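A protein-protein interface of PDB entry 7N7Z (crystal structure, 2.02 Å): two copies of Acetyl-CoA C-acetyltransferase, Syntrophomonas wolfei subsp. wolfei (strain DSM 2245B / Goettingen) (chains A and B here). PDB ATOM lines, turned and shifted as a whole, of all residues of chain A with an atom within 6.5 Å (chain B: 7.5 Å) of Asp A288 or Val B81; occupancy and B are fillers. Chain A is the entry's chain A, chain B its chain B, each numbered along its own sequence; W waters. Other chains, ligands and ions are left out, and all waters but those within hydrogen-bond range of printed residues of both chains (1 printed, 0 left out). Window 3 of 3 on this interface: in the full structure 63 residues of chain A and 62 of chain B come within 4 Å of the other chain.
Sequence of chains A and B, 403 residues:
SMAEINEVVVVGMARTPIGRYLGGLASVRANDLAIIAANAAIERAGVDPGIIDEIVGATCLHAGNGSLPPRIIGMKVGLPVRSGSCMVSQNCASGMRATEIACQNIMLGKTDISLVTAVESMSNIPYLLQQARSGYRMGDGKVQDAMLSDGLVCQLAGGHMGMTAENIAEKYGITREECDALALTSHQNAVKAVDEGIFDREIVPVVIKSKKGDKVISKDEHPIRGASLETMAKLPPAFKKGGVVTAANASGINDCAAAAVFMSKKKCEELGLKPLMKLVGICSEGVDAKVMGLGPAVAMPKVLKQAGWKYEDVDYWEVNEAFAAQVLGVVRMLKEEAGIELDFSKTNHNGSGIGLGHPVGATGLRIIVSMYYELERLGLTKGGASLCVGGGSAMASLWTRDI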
ATOM      1  N   LEU A 156      -5.451 -14.412  -9.662  1.00  0.00           N
ATOM      2  CA  LEU A 156      -6.835 -14.583  -9.230  1.00  0.00           C
ATOM      3  C   LEU A 156      -6.923 -14.743  -7.718  1.00  0.00           C
ATOM      4  O   LEU A 156      -7.789 -14.142  -7.070  1.00  0.00           O
ATOM      5  CB  LEU A 156      -7.459 -15.793  -9.926  1.00  0.00           C
ATOM      6  CG  LEU A 156      -7.327 -15.863 -11.448  1.00  0.00           C
ATOM      7  CD1 LEU A 156      -7.708 -17.247 -11.944  1.00  0.00           C
ATOM      8  CD2 LEU A 156      -8.183 -14.799 -12.117  1.00  0.00           C
ATOM      9  N   GLU A 285     -12.301 -30.869 -12.426  1.00  0.00           N
ATOM     10  CA  GLU A 285     -13.392 -30.149 -11.780  1.00  0.00           C
ATOM     11  C   GLU A 285     -12.812 -29.058 -10.889  1.00  0.00           C
ATOM     12  O   GLU A 285     -11.964 -29.331 -10.033  1.00  0.00           O
ATOM     13  CB  GLU A 285     -14.275 -31.104 -10.975  1.00  0.00           C
ATOM     14  CG  GLU A 285     -15.537 -30.456 -10.413  1.00  0.00           C
ATOM     15  CD  GLU A 285     -16.641 -30.321 -11.446  1.00  0.00           C
ATOM     16  OE1 GLU A 285     -16.533 -30.952 -12.518  1.00  0.00           O
ATOM     17  OE2 GLU A 285     -17.628 -29.600 -11.180  1.00  0.00           O
ATOM     18  N   GLY A 286     -13.266 -27.822 -11.082  1.00  0.00           N
ATOM     19  CA  GLY A 286     -12.647 -26.676 -10.461  1.00  0.00           C
ATOM     20  C   GLY A 286     -13.409 -26.132  -9.268  1.00  0.00           C
ATOM     21  O   GLY A 286     -14.585 -26.418  -9.062  1.00  0.00           O
ATOM     22  N   VAL A 287     -12.692 -25.341  -8.469  1.00  0.00           N
ATOM     23  CA  VAL A 287     -13.266 -24.543  -7.397  1.00  0.00           C
ATOM     24  C   VAL A 287     -12.711 -23.129  -7.535  1.00  0.00           C
ATOM     25  O   VAL A 287     -11.833 -22.861  -8.356  1.00  0.00           O
ATOM     26  CB  VAL A 287     -12.961 -25.118  -5.998  1.00  0.00           C
ATOM     27  CG1 VAL A 287     -13.463 -26.552  -5.888  1.00  0.00           C
ATOM     28  CG2 VAL A 287     -11.470 -25.045  -5.700  1.00  0.00           C
ATOM     29  N   ASP A 288     -13.237 -22.220  -6.719  1.00  0.00           N
ATOM     30  CA  ASP A 288     -12.766 -20.843  -6.753  1.00  0.00           C
ATOM     31  C   ASP A 288     -11.265 -20.791  -6.496  1.00  0.00           C
ATOM     32  O   ASP A 288     -10.723 -21.569  -5.705  1.00  0.00           O
ATOM     33  CB  ASP A 288     -13.510 -20.000  -5.717  1.00  0.00           C
ATOM     34  CG  ASP A 288     -13.284 -18.512  -5.908  1.00  0.00           C
ATOM     35  OD1 ASP A 288     -12.142 -18.053  -5.693  1.00  0.00           O
ATOM     36  OD2 ASP A 288     -14.245 -17.804  -6.276  1.00  0.00           O
ATOM     37  N   ALA A 289     -10.589 -19.861  -7.176  1.00  0.00           N
ATOM     38  CA  ALA A 289      -9.135 -19.788  -7.083  1.00  0.00           C
ATOM     39  C   ALA A 289      -8.675 -19.472  -5.666  1.00  0.00           C
ATOM     40  O   ALA A 289      -7.606 -19.930  -5.246  1.00  0.00           O
ATOM     41  CB  ALA A 289      -8.599 -18.737  -8.055  1.00  0.00           C
ATOM     42  N   LYS A 290      -9.455 -18.690  -4.919  1.00  0.00           N
ATOM     43  CA  LYS A 290      -9.055 -18.326  -3.565  1.00  0.00           C
ATOM     44  C   LYS A 290      -8.953 -19.538  -2.651  1.00  0.00           C
ATOM     45  O   LYS A 290      -8.214 -19.493  -1.661  1.00  0.00           O
ATOM     46  CB  LYS A 290     -10.043 -17.314  -2.984  1.00  0.00           C
ATOM     47  CG  LYS A 290      -9.694 -15.864  -3.288  1.00  0.00           C
ATOM     48  CD  LYS A 290     -10.127 -15.466  -4.690  1.00  0.00           C
ATOM     49  CE  LYS A 290     -11.589 -15.057  -4.726  1.00  0.00           C
ATOM     50  NZ  LYS A 290     -11.986 -14.528  -6.059  1.00  0.00           N
ATOM     51  N   VAL A 291      -9.670 -20.617  -2.960  1.00  0.00           N
ATOM     52  CA  VAL A 291      -9.619 -21.842  -2.170  1.00  0.00           C
ATOM     53  C   VAL A 291      -9.390 -23.021  -3.105  1.00  0.00           C
ATOM     54  O   VAL A 291     -10.077 -24.045  -3.013  1.00  0.00           O
ATOM     55  CB  VAL A 291     -10.908 -22.031  -1.348  1.00  0.00           C
ATOM     56  CG1 VAL A 291     -10.930 -21.069  -0.170  1.00  0.00           C
ATOM     57  CG2 VAL A 291     -12.134 -21.836  -2.228  1.00  0.00           C
ATOM     58  N   MET A 292      -8.423 -22.885  -4.016  1.00  0.00           N
ATOM     59  CA  MET A 292      -8.152 -23.958  -4.966  1.00  0.00           C
ATOM     60  C   MET A 292      -7.769 -25.259  -4.273  1.00  0.00           C
ATOM     61  O   MET A 292      -7.881 -26.327  -4.882  1.00  0.00           O
ATOM     62  CB  MET A 292      -7.044 -23.550  -5.946  1.00  0.00           C
ATOM     63  CG  MET A 292      -5.897 -22.738  -5.353  1.00  0.00           C
ATOM     64  SD  MET A 292      -4.994 -23.579  -4.043  1.00  0.00           S
ATOM     65  CE  MET A 292      -4.327 -24.987  -4.930  1.00  0.00           C
ATOM     66  N   GLY A 293      -7.325 -25.195  -3.015  1.00  0.00           N
ATOM     67  CA  GLY A 293      -6.951 -26.408  -2.309  1.00  0.00           C
ATOM     68  C   GLY A 293      -8.103 -27.375  -2.123  1.00  0.00           C
ATOM     69  O   GLY A 293      -7.890 -28.584  -2.005  1.00  0.00           O
ATOM     70  N   GLY A 391      -5.101 -22.072  -9.351  1.00  0.00           N
ATOM     71  CA  GLY A 391      -6.184 -21.582 -10.178  1.00  0.00           C
ATOM     72  C   GLY A 391      -7.506 -22.228  -9.817  1.00  0.00           C
ATOM     73  O   GLY A 391      -8.541 -21.557  -9.774  1.00  0.00           O
ATOM     74  N   GLY A 392      -7.485 -23.537  -9.565  1.00  0.00           N
ATOM     75  CA  GLY A 392      -8.658 -24.215  -9.051  1.00  0.00           C
ATOM     76  C   GLY A 392      -9.055 -25.477  -9.787  1.00  0.00           C
ATOM     77  O   GLY A 392      -9.713 -26.346  -9.207  1.00  0.00           O
ATOM     78  N   SER A 393      -8.666 -25.603 -11.055  1.00  0.00           N
ATOM     79  CA  SER A 393      -9.110 -26.742 -11.852  1.00  0.00           C
ATOM     80  C   SER A 393      -8.418 -28.032 -11.427  1.00  0.00           C
ATOM     81  O   SER A 393      -7.392 -28.412 -12.001  1.00  0.00           O
ATOM     82  CB  SER A 393      -8.867 -26.481 -13.341  1.00  0.00           C
ATOM     83  OG  SER A 393      -9.516 -25.293 -13.770  1.00  0.00           O
ATOM     84  N   GLY B  50     -21.243 -18.527 -18.259  1.00  0.00           N
ATOM     85  CA  GLY B  50     -21.315 -19.217 -16.984  1.00  0.00           C
ATOM     86  C   GLY B  50     -21.512 -20.717 -17.079  1.00  0.00           C
ATOM     87  O   GLY B  50     -21.368 -21.402 -16.061  1.00  0.00           O
ATOM     88  N   ILE B  52     -19.990 -22.592 -19.735  1.00  0.00           N
ATOM     89  CA  ILE B  52     -18.890 -23.196 -20.477  1.00  0.00           C
ATOM     90  C   ILE B  52     -18.113 -24.118 -19.547  1.00  0.00           C
ATOM     91  O   ILE B  52     -17.795 -23.753 -18.408  1.00  0.00           O
ATOM     92  CB  ILE B  52     -17.992 -22.109 -21.087  1.00  0.00           C
ATOM     93  CG1 ILE B  52     -18.769 -21.337 -22.161  1.00  0.00           C
ATOM     94  CG2 ILE B  52     -16.723 -22.725 -21.668  1.00  0.00           C
ATOM     95  CD1 ILE B  52     -18.015 -20.159 -22.759  1.00  0.00           C
ATOM     96  N   ASP B  53     -17.804 -25.323 -20.031  1.00  0.00           N
ATOM     97  CA  ASP B  53     -17.272 -26.361 -19.155  1.00  0.00           C
ATOM     98  C   ASP B  53     -15.772 -26.230 -18.926  1.00  0.00           C
ATOM     99  O   ASP B  53     -15.271 -26.677 -17.888  1.00  0.00           O
ATOM    100  CB  ASP B  53     -17.581 -27.742 -19.737  1.00  0.00           C
ATOM    101  CG  ASP B  53     -19.055 -28.077 -19.686  1.00  0.00           C
ATOM    102  OD1 ASP B  53     -19.673 -27.867 -18.621  1.00  0.00           O
ATOM    103  OD2 ASP B  53     -19.597 -28.548 -20.709  1.00  0.00           O
ATOM    104  N   ARG B  71      -6.588 -20.023 -17.341  1.00  0.00           N
ATOM    105  CA  ARG B  71      -7.504 -19.894 -16.214  1.00  0.00           C
ATOM    106  C   ARG B  71      -7.794 -18.428 -15.917  1.00  0.00           C
ATOM    107  O   ARG B  71      -8.926 -18.070 -15.569  1.00  0.00           O
ATOM    108  CB  ARG B  71      -6.925 -20.595 -14.983  1.00  0.00           C
ATOM    109  CG  ARG B  71      -7.748 -20.428 -13.706  1.00  0.00           C
ATOM    110  CD  ARG B  71      -9.134 -21.061 -13.815  1.00  0.00           C
ATOM    111  NE  ARG B  71      -9.749 -21.230 -12.502  1.00  0.00           N
ATOM    112  CZ  ARG B  71     -10.850 -21.932 -12.266  1.00  0.00           C
ATOM    113  NH1 ARG B  71     -11.507 -22.541 -13.242  1.00  0.00           N
ATOM    114  NH2 ARG B  71     -11.303 -22.027 -11.019  1.00  0.00           N
ATOM    115  N   MET B  75     -11.695 -17.009 -16.378  1.00  0.00           N
ATOM    116  CA  MET B  75     -12.412 -16.339 -15.300  1.00  0.00           C
ATOM    117  C   MET B  75     -12.796 -14.917 -15.683  1.00  0.00           C
ATOM    118  O   MET B  75     -13.862 -14.432 -15.286  1.00  0.00           O
ATOM    119  CB  MET B  75     -11.562 -16.331 -14.029  1.00  0.00           C
ATOM    120  CG  MET B  75     -11.304 -17.709 -13.441  1.00  0.00           C
ATOM    121  SD  MET B  75     -12.815 -18.590 -12.998  1.00  0.00           S
ATOM    122  CE  MET B  75     -13.045 -19.616 -14.449  1.00  0.00           C
ATOM    123  N   GLY B  78     -15.773 -14.828 -17.794  1.00  0.00           N
ATOM    124  CA  GLY B  78     -16.959 -15.270 -17.089  1.00  0.00           C
ATOM    125  C   GLY B  78     -17.198 -16.762 -17.055  1.00  0.00           C
ATOM    126  O   GLY B  78     -18.338 -17.180 -16.813  1.00  0.00           O
ATOM    127  N   LEU B  79     -16.175 -17.577 -17.289  1.00  0.00           N
ATOM    128  CA  LEU B  79     -16.344 -19.010 -17.120  1.00  0.00           C
ATOM    129  C   LEU B  79     -16.617 -19.314 -15.647  1.00  0.00           C
ATOM    130  O   LEU B  79     -16.153 -18.591 -14.760  1.00  0.00           O
ATOM    131  CB  LEU B  79     -15.103 -19.768 -17.588  1.00  0.00           C
ATOM    132  CG  LEU B  79     -15.214 -20.455 -18.951  1.00  0.00           C
ATOM    133  CD1 LEU B  79     -15.493 -19.438 -20.047  1.00  0.00           C
ATOM    134  CD2 LEU B  79     -13.951 -21.248 -19.261  1.00  0.00           C
ATOM    135  N   PRO B  80     -17.370 -20.370 -15.354  1.00  0.00           N
ATOM    136  CA  PRO B  80     -17.607 -20.725 -13.953  1.00  0.00           C
ATOM    137  C   PRO B  80     -16.352 -21.303 -13.320  1.00  0.00           C
ATOM    138  O   PRO B  80     -15.522 -21.926 -13.986  1.00  0.00           O
ATOM    139  CB  PRO B  80     -18.724 -21.769 -14.036  1.00  0.00           C
ATOM    140  CG  PRO B  80     -18.520 -22.413 -15.365  1.00  0.00           C
ATOM    141  CD  PRO B  80     -17.984 -21.339 -16.280  1.00  0.00           C
ATOM    142  N   VAL B  81     -16.217 -21.086 -12.008  1.00  0.00           N
ATOM    143  CA  VAL B  81     -15.043 -21.575 -11.296  1.00  0.00           C
ATOM    144  C   VAL B  81     -14.956 -23.093 -11.348  1.00  0.00           C
ATOM    145  O   VAL B  81     -13.878 -23.660 -11.133  1.00  0.00           O
ATOM    146  CB  VAL B  81     -15.047 -21.078  -9.833  1.00  0.00           C
ATOM    147  CG1 VAL B  81     -15.278 -19.574  -9.779  1.00  0.00           C
ATOM    148  CG2 VAL B  81     -16.097 -21.821  -9.015  1.00  0.00           C
ATOM    149  N   ARG B  82     -16.071 -23.773 -11.625  1.00  0.00           N
ATOM    150  CA  ARG B  82     -16.046 -25.222 -11.779  1.00  0.00           C
ATOM    151  C   ARG B  82     -15.386 -25.655 -13.081  1.00  0.00           C
ATOM    152  O   ARG B  82     -15.013 -26.825 -13.212  1.00  0.00           O
ATOM    153  CB  ARG B  82     -17.470 -25.784 -11.720  1.00  0.00           C
ATOM    154  CG  ARG B  82     -18.399 -25.243 -12.805  1.00  0.00           C
ATOM    155  CD  ARG B  82     -19.534 -26.212 -13.120  1.00  0.00           C
ATOM    156  NE  ARG B  82     -20.207 -25.873 -14.371  1.00  0.00           N
ATOM    157  CZ  ARG B  82     -20.051 -26.520 -15.520  1.00  0.00           C
ATOM    158  NH1 ARG B  82     -19.248 -27.567 -15.625  1.00  0.00           N
ATOM    159  NH2 ARG B  82     -20.717 -26.104 -16.593  1.00  0.00           N
ATOM    160  N   SER B  83     -15.233 -24.741 -14.036  1.00  0.00           N
ATOM    161  CA  SER B  83     -14.778 -25.105 -15.369  1.00  0.00           C
ATOM    162  C   SER B  83     -13.326 -25.573 -15.346  1.00  0.00           C
ATOM    163  O   SER B  83     -12.538 -25.217 -14.464  1.00  0.00           O
ATOM    164  CB  SER B  83     -14.923 -23.921 -16.327  1.00  0.00           C
ATOM    165  OG  SER B  83     -14.204 -22.791 -15.861  1.00  0.00           O
ATOM    166  N   GLY B  84     -12.978 -26.389 -16.343  1.00  0.00           N
ATOM    167  CA  GLY B  84     -11.615 -26.843 -16.484  1.00  0.00           C
ATOM    168  C   GLY B  84     -10.728 -25.811 -17.154  1.00  0.00           C
ATOM    169  O   GLY B  84     -11.187 -24.851 -17.771  1.00  0.00           O
HETATM  170  O   HOH W   1     -17.182 -28.626 -14.415  1.00  0.00           O
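Water W1 lies within hydrogen-bond range of the guanidinium group (NH1) of Arg B82 (2.6 Å) and the side-chain carboxylate (OE1) of Glu A285 (3.1 Å).
The side-chain carboxylate (OD1) of Asp A288 lies within salt-bridge range of the side-chain amino group (NZ) of Lys A290, at 3.5 Å. The backbone carbonyl oxygen of Gly A392 lies within hydrogen-bond range of the backbone NH of Val A287, 3.2 Å away. The backbone carbonyl oxygen of Asp B53 sits at hydrogen-bond distance from the backbone NH of Gly B84. The guanidinium group (NH2) of Arg B71 is in hydrogen-bond range of the backbone carbonyl oxygen (O) of Val B81. The backbone carbonyl oxygen (O) of Pro B80 sits at hydrogen-bond distance from the side-chain hydroxyl (OG) of Ser B83. The guanidinium group (NH1) of Arg B71 sits at hydrogen-bond distance from the backbone carbonyl oxygen (O) of Ser B83 (3.1 Å).
Leu A156 touches Arg B71. CG of Met B75 touches CD1 of Leu A156, at 3.9 Å. Glu A285 touches Arg B82. Gly A286 touches Val B81. Val B81 touches Asp A288 (CG2 to N, 3.7 Å). Gly A392 touches Arg B71 (CA to NH2, 3.96 Å). Ser A393 touches Gly B84 (OG to C, 3.6 Å).
The backbone NH (N) of Gly A286 sits at hydrogen-bond distance from the backbone carbonyl oxygen (O) of Arg B82 (2.9 Å). The guanidinium group (NH1) of Arg B71 sits at hydrogen-bond distance from the side-chain hydroxyl (OG) of Ser A393. The backbone carbonyl oxygen of Val B81 sits at hydrogen-bond distance from the backbone NH of Val A287 (3.4 Å). The side-chain hydroxyl (OG) of Ser A393 is in hydrogen-bond range of the backbone carbonyl oxygen (O) of Ser B83 (3.1 Å). O of Gly A391 sits at hydrogen-bond distance from NE of Arg B71 (3.0 Å). The guanidinium group of Arg B71 sits at hydrogen-bond distance from the backbone carbonyl oxygen of Val A287, at 2.8 Å.
No position is printed for both chains.
Hydrophobic or aromatic side chains of chain B that line the printed part of chain A: Met B75 and Val B81. Among the printed residues, 13 pairs touch across the chains. Among the printed residues, no Asp or Glu carboxylate lies within 4 Å of a Lys or Arg side-chain nitrogen of the other chain.
Of chain B, only Val B81 comes within 4 Å of Asp A288. Val B81 touches just these residues of chain A: Gly A286, Val A287 and Asp A288. Of the printed residues of chain B, Glu A285 touches Arg B82 (3.9 Å). Printed residues of chain B within 4 Å of Ser A393: Arg B71, Ser B83 and Gly B84.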
